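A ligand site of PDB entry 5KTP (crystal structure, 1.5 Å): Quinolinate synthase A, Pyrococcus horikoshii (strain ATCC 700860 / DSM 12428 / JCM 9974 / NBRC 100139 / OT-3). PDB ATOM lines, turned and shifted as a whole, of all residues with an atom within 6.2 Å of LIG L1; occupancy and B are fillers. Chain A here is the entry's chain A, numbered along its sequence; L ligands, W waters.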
ATOM      1  N   HIS A  25      38.179  29.983 -30.634  1.00  0.00           N
ATOM      2  CA  HIS A  25      36.961  30.646 -30.221  1.00  0.00           C
ATOM      3  C   HIS A  25      37.256  31.650 -29.091  1.00  0.00           C
ATOM      4  O   HIS A  25      38.238  31.513 -28.351  1.00  0.00           O
ATOM      5  CB  HIS A  25      35.908  29.638 -29.770  1.00  0.00           C
ATOM      6  CG  HIS A  25      34.586  30.277 -29.495  1.00  0.00           C
ATOM      7  ND1 HIS A  25      34.181  30.635 -28.235  1.00  0.00           N
ATOM      8  CD2 HIS A  25      33.610  30.676 -30.345  1.00  0.00           C
ATOM      9  CE1 HIS A  25      32.993  31.221 -28.316  1.00  0.00           C
ATOM     10  NE2 HIS A  25      32.623  31.245 -29.583  1.00  0.00           N
ATOM     11  N   TYR A  27      36.060  31.930 -26.274  1.00  0.00           N
ATOM     12  CA  TYR A  27      36.016  31.361 -24.927  1.00  0.00           C
ATOM     13  C   TYR A  27      37.265  30.561 -24.597  1.00  0.00           C
ATOM     14  O   TYR A  27      37.334  29.964 -23.515  1.00  0.00           O
ATOM     15  CB  TYR A  27      34.808  30.443 -24.735  1.00  0.00           C
ATOM     16  CG  TYR A  27      33.427  31.078 -24.890  1.00  0.00           C
ATOM     17  CD1 TYR A  27      33.255  32.451 -24.799  1.00  0.00           C
ATOM     18  CD2 TYR A  27      32.311  30.277 -25.118  1.00  0.00           C
ATOM     19  CE1 TYR A  27      31.989  33.014 -24.939  1.00  0.00           C
ATOM     20  CE2 TYR A  27      31.052  30.834 -25.263  1.00  0.00           C
ATOM     21  CZ  TYR A  27      30.898  32.191 -25.169  1.00  0.00           C
ATOM     22  OH  TYR A  27      29.657  32.760 -25.324  1.00  0.00           O
ATOM     23  N   VAL A  62      35.246  23.772 -29.710  1.00  0.00           N
ATOM     24  CA  VAL A  62      34.562  22.498 -29.450  1.00  0.00           C
ATOM     25  C   VAL A  62      34.278  21.747 -30.753  1.00  0.00           C
ATOM     26  O   VAL A  62      34.434  22.300 -31.844  1.00  0.00           O
ATOM     27  CB  VAL A  62      33.264  22.717 -28.653  1.00  0.00           C
ATOM     28  CG1 VAL A  62      33.608  23.243 -27.251  1.00  0.00           C
ATOM     29  CG2 VAL A  62      32.353  23.682 -29.366  1.00  0.00           C
ATOM     30  N   PHE A  64      31.736  20.648 -32.603  1.00  0.00           N
ATOM     31  CA  PHE A  64      30.869  21.086 -33.700  1.00  0.00           C
ATOM     32  C   PHE A  64      31.516  22.212 -34.503  1.00  0.00           C
ATOM     33  O   PHE A  64      31.227  22.358 -35.698  1.00  0.00           O
ATOM     34  CB  PHE A  64      29.467  21.493 -33.184  1.00  0.00           C
ATOM     35  CG  PHE A  64      29.379  22.860 -32.514  1.00  0.00           C
ATOM     36  CD1 PHE A  64      29.311  24.040 -33.257  1.00  0.00           C
ATOM     37  CD2 PHE A  64      29.286  22.951 -31.133  1.00  0.00           C
ATOM     38  CE1 PHE A  64      29.216  25.274 -32.628  1.00  0.00           C
ATOM     39  CE2 PHE A  64      29.184  24.191 -30.499  1.00  0.00           C
ATOM     40  CZ  PHE A  64      29.155  25.347 -31.243  1.00  0.00           C
ATOM     41  N   MET A  65      32.384  22.993 -33.871  1.00  0.00           N
ATOM     42  CA  MET A  65      33.060  24.069 -34.575  1.00  0.00           C
ATOM     43  C   MET A  65      34.123  23.527 -35.510  1.00  0.00           C
ATOM     44  O   MET A  65      34.234  23.971 -36.659  1.00  0.00           O
ATOM     45  CB  MET A  65      33.677  25.043 -33.584  1.00  0.00           C
ATOM     46  CG  MET A  65      32.689  25.679 -32.633  1.00  0.00           C
ATOM     47  SD  MET A  65      33.464  26.806 -31.434  1.00  0.00           S
ATOM     48  CE  MET A  65      31.968  27.421 -30.648  1.00  0.00           C
ATOM     49  N   THR A  86      33.583  19.384 -26.194  1.00  0.00           N
ATOM     50  CA  THR A  86      32.257  19.165 -26.751  1.00  0.00           C
ATOM     51  C   THR A  86      31.284  20.199 -26.201  1.00  0.00           C
ATOM     52  O   THR A  86      31.523  20.824 -25.164  1.00  0.00           O
ATOM     53  CB  THR A  86      31.729  17.753 -26.445  1.00  0.00           C
ATOM     54  OG1 THR A  86      31.564  17.615 -25.020  1.00  0.00           O
ATOM     55  CG2 THR A  86      32.686  16.673 -26.942  1.00  0.00           C
ATOM     56  N   CYS A  87      30.143  20.332 -26.889  1.00  0.00           N
ATOM     57  CA  CYS A  87      29.112  21.306 -26.558  1.00  0.00           C
ATOM     58  C   CYS A  87      27.886  20.584 -26.016  1.00  0.00           C
ATOM     59  O   CYS A  87      27.212  19.844 -26.758  1.00  0.00           O
ATOM     60  CB  CYS A  87      28.736  22.148 -27.771  1.00  0.00           C
ATOM     61  SG  CYS A  87      27.344  23.279 -27.504  1.00  0.00           S
ATOM     62  N   ALA A  88      27.571  20.816 -24.736  1.00  0.00           N
ATOM     63  CA  ALA A  88      26.446  20.143 -24.110  1.00  0.00           C
ATOM     64  C   ALA A  88      25.126  20.532 -24.765  1.00  0.00           C
ATOM     65  O   ALA A  88      24.218  19.705 -24.882  1.00  0.00           O
ATOM     66  CB  ALA A  88      26.419  20.462 -22.611  1.00  0.00           C
ATOM     67  N   MET A  89      25.002  21.794 -25.204  1.00  0.00           N
ATOM     68  CA  MET A  89      23.768  22.212 -25.857  1.00  0.00           C
ATOM     69  C   MET A  89      23.596  21.525 -27.204  1.00  0.00           C
ATOM     70  O   MET A  89      22.520  20.993 -27.504  1.00  0.00           O
ATOM     71  CB  MET A  89      23.734  23.739 -26.003  1.00  0.00           C
ATOM     72  CG  MET A  89      22.412  24.276 -26.583  1.00  0.00           C
ATOM     73  SD  MET A  89      22.649  24.852 -28.271  1.00  0.00           S
ATOM     74  CE  MET A  89      23.625  26.312 -27.926  1.00  0.00           C
ATOM     75  N   ALA A  90      24.663  21.497 -28.006  1.00  0.00           N
ATOM     76  CA  ALA A  90      24.564  20.924 -29.344  1.00  0.00           C
ATOM     77  C   ALA A  90      24.195  19.442 -29.273  1.00  0.00           C
ATOM     78  O   ALA A  90      23.431  18.935 -30.099  1.00  0.00           O
ATOM     79  CB  ALA A  90      25.873  21.125 -30.096  1.00  0.00           C
ATOM     80  N   TYR A 113      20.826  26.049 -35.483  1.00  0.00           N
ATOM     81  CA  TYR A 113      21.986  26.701 -34.894  1.00  0.00           C
ATOM     82  C   TYR A 113      23.243  25.967 -35.334  1.00  0.00           C
ATOM     83  O   TYR A 113      23.253  24.726 -35.432  1.00  0.00           O
ATOM     84  CB  TYR A 113      21.856  26.658 -33.365  1.00  0.00           C
ATOM     85  CG  TYR A 113      22.436  27.793 -32.531  1.00  0.00           C
ATOM     86  CD1 TYR A 113      22.981  28.940 -33.108  1.00  0.00           C
ATOM     87  CD2 TYR A 113      22.418  27.708 -31.151  1.00  0.00           C
ATOM     88  CE1 TYR A 113      23.504  29.957 -32.297  1.00  0.00           C
ATOM     89  CE2 TYR A 113      22.915  28.691 -30.359  1.00  0.00           C
ATOM     90  CZ  TYR A 113      23.462  29.817 -30.929  1.00  0.00           C
ATOM     91  OH  TYR A 113      23.949  30.780 -30.084  1.00  0.00           O
ATOM     92  N   ASN A 115      25.535  25.532 -33.520  1.00  0.00           N
ATOM     93  CA  ASN A 115      25.769  24.675 -32.361  1.00  0.00           C
ATOM     94  C   ASN A 115      24.955  23.395 -32.546  1.00  0.00           C
ATOM     95  O   ASN A 115      23.913  23.192 -31.916  1.00  0.00           O
ATOM     96  CB  ASN A 115      25.394  25.391 -31.064  1.00  0.00           C
ATOM     97  CG  ASN A 115      26.159  26.694 -30.851  1.00  0.00           C
ATOM     98  OD1 ASN A 115      26.318  27.488 -31.761  1.00  0.00           O
ATOM     99  ND2 ASN A 115      26.637  26.906 -29.623  1.00  0.00           N
ATOM    100  N   ASP A 150      18.768  25.701 -29.259  1.00  0.00           N
ATOM    101  CA  ASP A 150      18.705  26.543 -28.067  1.00  0.00           C
ATOM    102  C   ASP A 150      17.348  27.239 -27.950  1.00  0.00           C
ATOM    103  O   ASP A 150      16.998  28.077 -28.771  1.00  0.00           O
ATOM    104  CB  ASP A 150      19.834  27.569 -28.081  1.00  0.00           C
ATOM    105  CG  ASP A 150      20.029  28.227 -26.730  1.00  0.00           C
ATOM    106  OD1 ASP A 150      20.960  27.825 -26.000  1.00  0.00           O
ATOM    107  OD2 ASP A 150      19.229  29.130 -26.388  1.00  0.00           O
ATOM    108  N   CYS A 174      21.981  26.011 -22.985  1.00  0.00           N
ATOM    109  CA  CYS A 174      23.379  26.024 -22.585  1.00  0.00           C
ATOM    110  C   CYS A 174      23.481  26.194 -21.065  1.00  0.00           C
ATOM    111  O   CYS A 174      23.072  27.245 -20.536  1.00  0.00           O
ATOM    112  CB  CYS A 174      24.117  27.159 -23.291  1.00  0.00           C
ATOM    113  SG  CYS A 174      25.737  27.519 -22.593  1.00  0.00           S
ATOM    114  N   TYR A 175      24.047  25.201 -20.364  1.00  0.00           N
ATOM    115  CA  TYR A 175      24.141  25.295 -18.911  1.00  0.00           C
ATOM    116  C   TYR A 175      24.982  26.493 -18.470  1.00  0.00           C
ATOM    117  O   TYR A 175      24.763  27.026 -17.385  1.00  0.00           O
ATOM    118  CB  TYR A 175      24.726  24.017 -18.287  1.00  0.00           C
ATOM    119  CG  TYR A 175      26.201  23.770 -18.535  1.00  0.00           C
ATOM    120  CD1 TYR A 175      27.157  24.142 -17.595  1.00  0.00           C
ATOM    121  CD2 TYR A 175      26.631  23.159 -19.692  1.00  0.00           C
ATOM    122  CE1 TYR A 175      28.513  23.902 -17.810  1.00  0.00           C
ATOM    123  CE2 TYR A 175      27.977  22.929 -19.932  1.00  0.00           C
ATOM    124  CZ  TYR A 175      28.918  23.305 -18.976  1.00  0.00           C
ATOM    125  OH  TYR A 175      30.260  23.068 -19.192  1.00  0.00           O
ATOM    126  N   VAL A 176      25.963  26.907 -19.284  1.00  0.00           N
ATOM    127  CA  VAL A 176      26.784  28.041 -18.900  1.00  0.00           C
ATOM    128  C   VAL A 176      25.948  29.298 -18.835  1.00  0.00           C
ATOM    129  O   VAL A 176      25.953  30.015 -17.816  1.00  0.00           O
ATOM    130  CB  VAL A 176      27.968  28.219 -19.862  1.00  0.00           C
ATOM    131  CG1 VAL A 176      28.802  29.443 -19.441  1.00  0.00           C
ATOM    132  CG2 VAL A 176      28.817  26.931 -19.896  1.00  0.00           C
ATOM    133  N   HIS A 177      25.218  29.598 -19.910  1.00  0.00           N
ATOM    134  CA  HIS A 177      24.423  30.824 -19.938  1.00  0.00           C
ATOM    135  C   HIS A 177      23.167  30.731 -19.092  1.00  0.00           C
ATOM    136  O   HIS A 177      22.660  31.771 -18.667  1.00  0.00           O
ATOM    137  CB  HIS A 177      24.082  31.187 -21.375  1.00  0.00           C
ATOM    138  CG  HIS A 177      25.266  31.666 -22.148  1.00  0.00           C
ATOM    139  ND1 HIS A 177      26.065  30.819 -22.888  1.00  0.00           N
ATOM    140  CD2 HIS A 177      25.841  32.894 -22.237  1.00  0.00           C
ATOM    141  CE1 HIS A 177      27.054  31.512 -23.436  1.00  0.00           C
ATOM    142  NE2 HIS A 177      26.923  32.780 -23.062  1.00  0.00           N
ATOM    143  N   GLU A 202      21.749  33.327 -25.460  1.00  0.00           N
ATOM    144  CA  GLU A 202      21.566  32.032 -24.808  1.00  0.00           C
ATOM    145  C   GLU A 202      21.166  32.170 -23.329  1.00  0.00           C
ATOM    146  O   GLU A 202      20.830  31.158 -22.701  1.00  0.00           O
ATOM    147  CB  GLU A 202      22.844  31.181 -24.938  1.00  0.00           C
ATOM    148  CG  GLU A 202      23.055  30.699 -26.363  1.00  0.00           C
ATOM    149  CD  GLU A 202      24.374  29.975 -26.565  1.00  0.00           C
ATOM    150  OE1 GLU A 202      25.051  29.659 -25.564  1.00  0.00           O
ATOM    151  OE2 GLU A 202      24.728  29.721 -27.724  1.00  0.00           O
ATOM    152  N   GLU A 235      30.292  33.487 -21.180  1.00  0.00           N
ATOM    153  CA  GLU A 235      31.398  32.717 -20.629  1.00  0.00           C
ATOM    154  C   GLU A 235      32.554  33.635 -20.251  1.00  0.00           C
ATOM    155  O   GLU A 235      32.906  34.537 -21.017  1.00  0.00           O
ATOM    156  CB  GLU A 235      31.846  31.653 -21.647  1.00  0.00           C
ATOM    157  CG  GLU A 235      32.330  30.362 -21.045  1.00  0.00           C
ATOM    158  CD  GLU A 235      33.817  30.359 -20.751  1.00  0.00           C
ATOM    159  OE1 GLU A 235      34.321  29.328 -20.258  1.00  0.00           O
ATOM    160  OE2 GLU A 235      34.485  31.385 -21.035  1.00  0.00           O
ATOM    161  N   CYS A 260      32.708  27.157 -19.441  1.00  0.00           N
ATOM    162  CA  CYS A 260      32.386  26.044 -20.335  1.00  0.00           C
ATOM    163  C   CYS A 260      33.466  24.969 -20.192  1.00  0.00           C
ATOM    164  O   CYS A 260      34.588  25.160 -20.672  1.00  0.00           O
ATOM    165  CB  CYS A 260      32.296  26.499 -21.779  1.00  0.00           C
ATOM    166  SG  CYS A 260      31.928  25.108 -22.870  1.00  0.00           S
ATOM    167  N   ILE A 261      33.103  23.832 -19.602  1.00  0.00           N
ATOM    168  CA  ILE A 261      34.066  22.744 -19.417  1.00  0.00           C
ATOM    169  C   ILE A 261      34.586  22.252 -20.774  1.00  0.00           C
ATOM    170  O   ILE A 261      35.771  21.989 -20.930  1.00  0.00           O
ATOM    171  CB  ILE A 261      33.437  21.611 -18.583  1.00  0.00           C
ATOM    172  CG1 ILE A 261      33.150  22.121 -17.150  1.00  0.00           C
ATOM    173  CG2 ILE A 261      34.334  20.387 -18.498  1.00  0.00           C
ATOM    174  CD1 ILE A 261      32.422  21.147 -16.264  1.00  0.00           C
ATOM    175  N   GLY A 262      33.711  22.149 -21.770  1.00  0.00           N
ATOM    176  CA  GLY A 262      34.152  21.687 -23.084  1.00  0.00           C
ATOM    177  C   GLY A 262      35.210  22.577 -23.704  1.00  0.00           C
ATOM    178  O   GLY A 262      36.236  22.104 -24.211  1.00  0.00           O
ATOM    179  N   MET A 263      34.975  23.895 -23.658  1.00  0.00           N
ATOM    180  CA  MET A 263      35.967  24.838 -24.183  1.00  0.00           C
ATOM    181  C   MET A 263      37.314  24.657 -23.482  1.00  0.00           C
ATOM    182  O   MET A 263      38.374  24.693 -24.120  1.00  0.00           O
ATOM    183  CB  MET A 263      35.462  26.270 -24.002  1.00  0.00           C
ATOM    184  CG  MET A 263      34.405  26.682 -25.002  1.00  0.00           C
ATOM    185  SD  MET A 263      35.106  26.826 -26.660  1.00  0.00           S
ATOM    186  CE  MET A 263      33.623  27.211 -27.599  1.00  0.00           C
HETATM  187 FE1  LIG L   1      28.116  24.809 -25.865  1.00  0.00          FE
HETATM  188 FE2  LIG L   1      29.974  25.607 -24.121  1.00  0.00          FE
HETATM  189 FE3  LIG L   1      27.437  26.557 -23.975  1.00  0.00          FE
HETATM  190 FE4  LIG L   1      28.988  27.255 -26.026  1.00  0.00          FE
HETATM  191  S1  LIG L   1      29.309  27.736 -23.817  1.00  0.00           S
HETATM  192  S2  LIG L   1      26.797  26.603 -26.104  1.00  0.00           S
HETATM  193  S3  LIG L   1      30.253  25.400 -26.290  1.00  0.00           S
HETATM  194  S4  LIG L   1      28.073  24.387 -23.653  1.00  0.00           S
HETATM  195  C1  LG2 L   2      29.352  32.947 -29.470  1.00  0.00           C
HETATM  196  C2  LG2 L   2      28.929  31.503 -29.436  1.00  0.00           C
HETATM  197  C3  LG2 L   2      27.749  31.268 -30.331  1.00  0.00           C
HETATM  198  C4  LG2 L   2      27.572  31.969 -31.622  1.00  0.00           C
HETATM  199  O1  LG2 L   2      26.527  31.818 -32.239  1.00  0.00           O
HETATM  200  O2  LG2 L   2      28.449  32.699 -32.079  1.00  0.00           O
HETATM  201  C5  LG2 L   2      26.846  30.383 -29.916  1.00  0.00           C
HETATM  202  O3  LG2 L   2      30.534  33.184 -29.633  1.00  0.00           O
HETATM  203  O4  LG2 L   2      28.524  33.838 -29.340  1.00  0.00           O
HETATM  204  O   HOH W   1      28.052  30.152 -26.723  1.00  0.00           O
HETATM  205  O   HOH W   2      29.691  28.556 -27.825  1.00  0.00           O
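Water W1 bridges OE1 of Glu 202 and OH of Tyr 27.
S2 of LIG L1 sits close to OE1 of Glu 202, at 3.6 Å. CE2 of Tyr 27 touches S1 of LIG L1, at 3.8 Å. Met 89 touches LIG L1. CE2 of Tyr 175 touches S4 of LIG L1 (3.998 Å). Hydrophobic or aromatic side chains within 4 Å of LIG L1: Tyr 27, Met 89 and Tyr 175. Within 4 Å of LIG L1: Tyr 27, Cys 87, Ala 88, Met 89, Asn 115, Cys 174, Tyr 175, Glu 202 and Cys 260. The nearest printed residue that does not touch LIG L1 is Val 176 (4.03 Å).
The side-chain hydroxyl (OH) of Tyr 175 lies within hydrogen-bond range of the backbone NH (N) of Ile 261. The side-chain sulfur (SG) of Cys 87 sits close to the backbone NH (N) of Met 89. The backbone NH (N) of Val 176 lies close to the side-chain sulfur (SG) of Cys 174, 3.4 Å away. The side-chain carboxylate (OE2) of Glu 202 lies within hydrogen-bond range of the side-chain hydroxyl (OH) of Tyr 113 (2.7 Å). N of Tyr 27 lies within hydrogen-bond range of ND1 of His 25, at 3.0 Å. The backbone NH of Gly 262 sits close to the side-chain sulfur of Cys 260 (3.6 Å). N of Ala 90 sits close to SG of Cys 87 (3.3 Å). SG of Cys 174 sits close to OE1 of Glu 202 (3.7 Å).
N of Ala 88 sits close to S4 of LIG L1, at 3.8 Å. An iron atom (FE1) of LIG L1 is bound by the side-chain sulfur (SG) of Cys 87. The side-chain sulfur of Cys 174 is bound to an iron atom (FE3) of LIG L1 (2.4 Å). The side-chain amide nitrogen (ND2) of Asn 115 sits close to a sulfur (S2) of LIG L1 (3.5 Å). The side-chain sulfur (SG) of Cys 260 is bound to an iron atom (FE2) of LIG L1 (2.4 Å). NE2 of His 25 is in hydrogen-bond range of O3 of LG2 L2 (2.9 Å).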
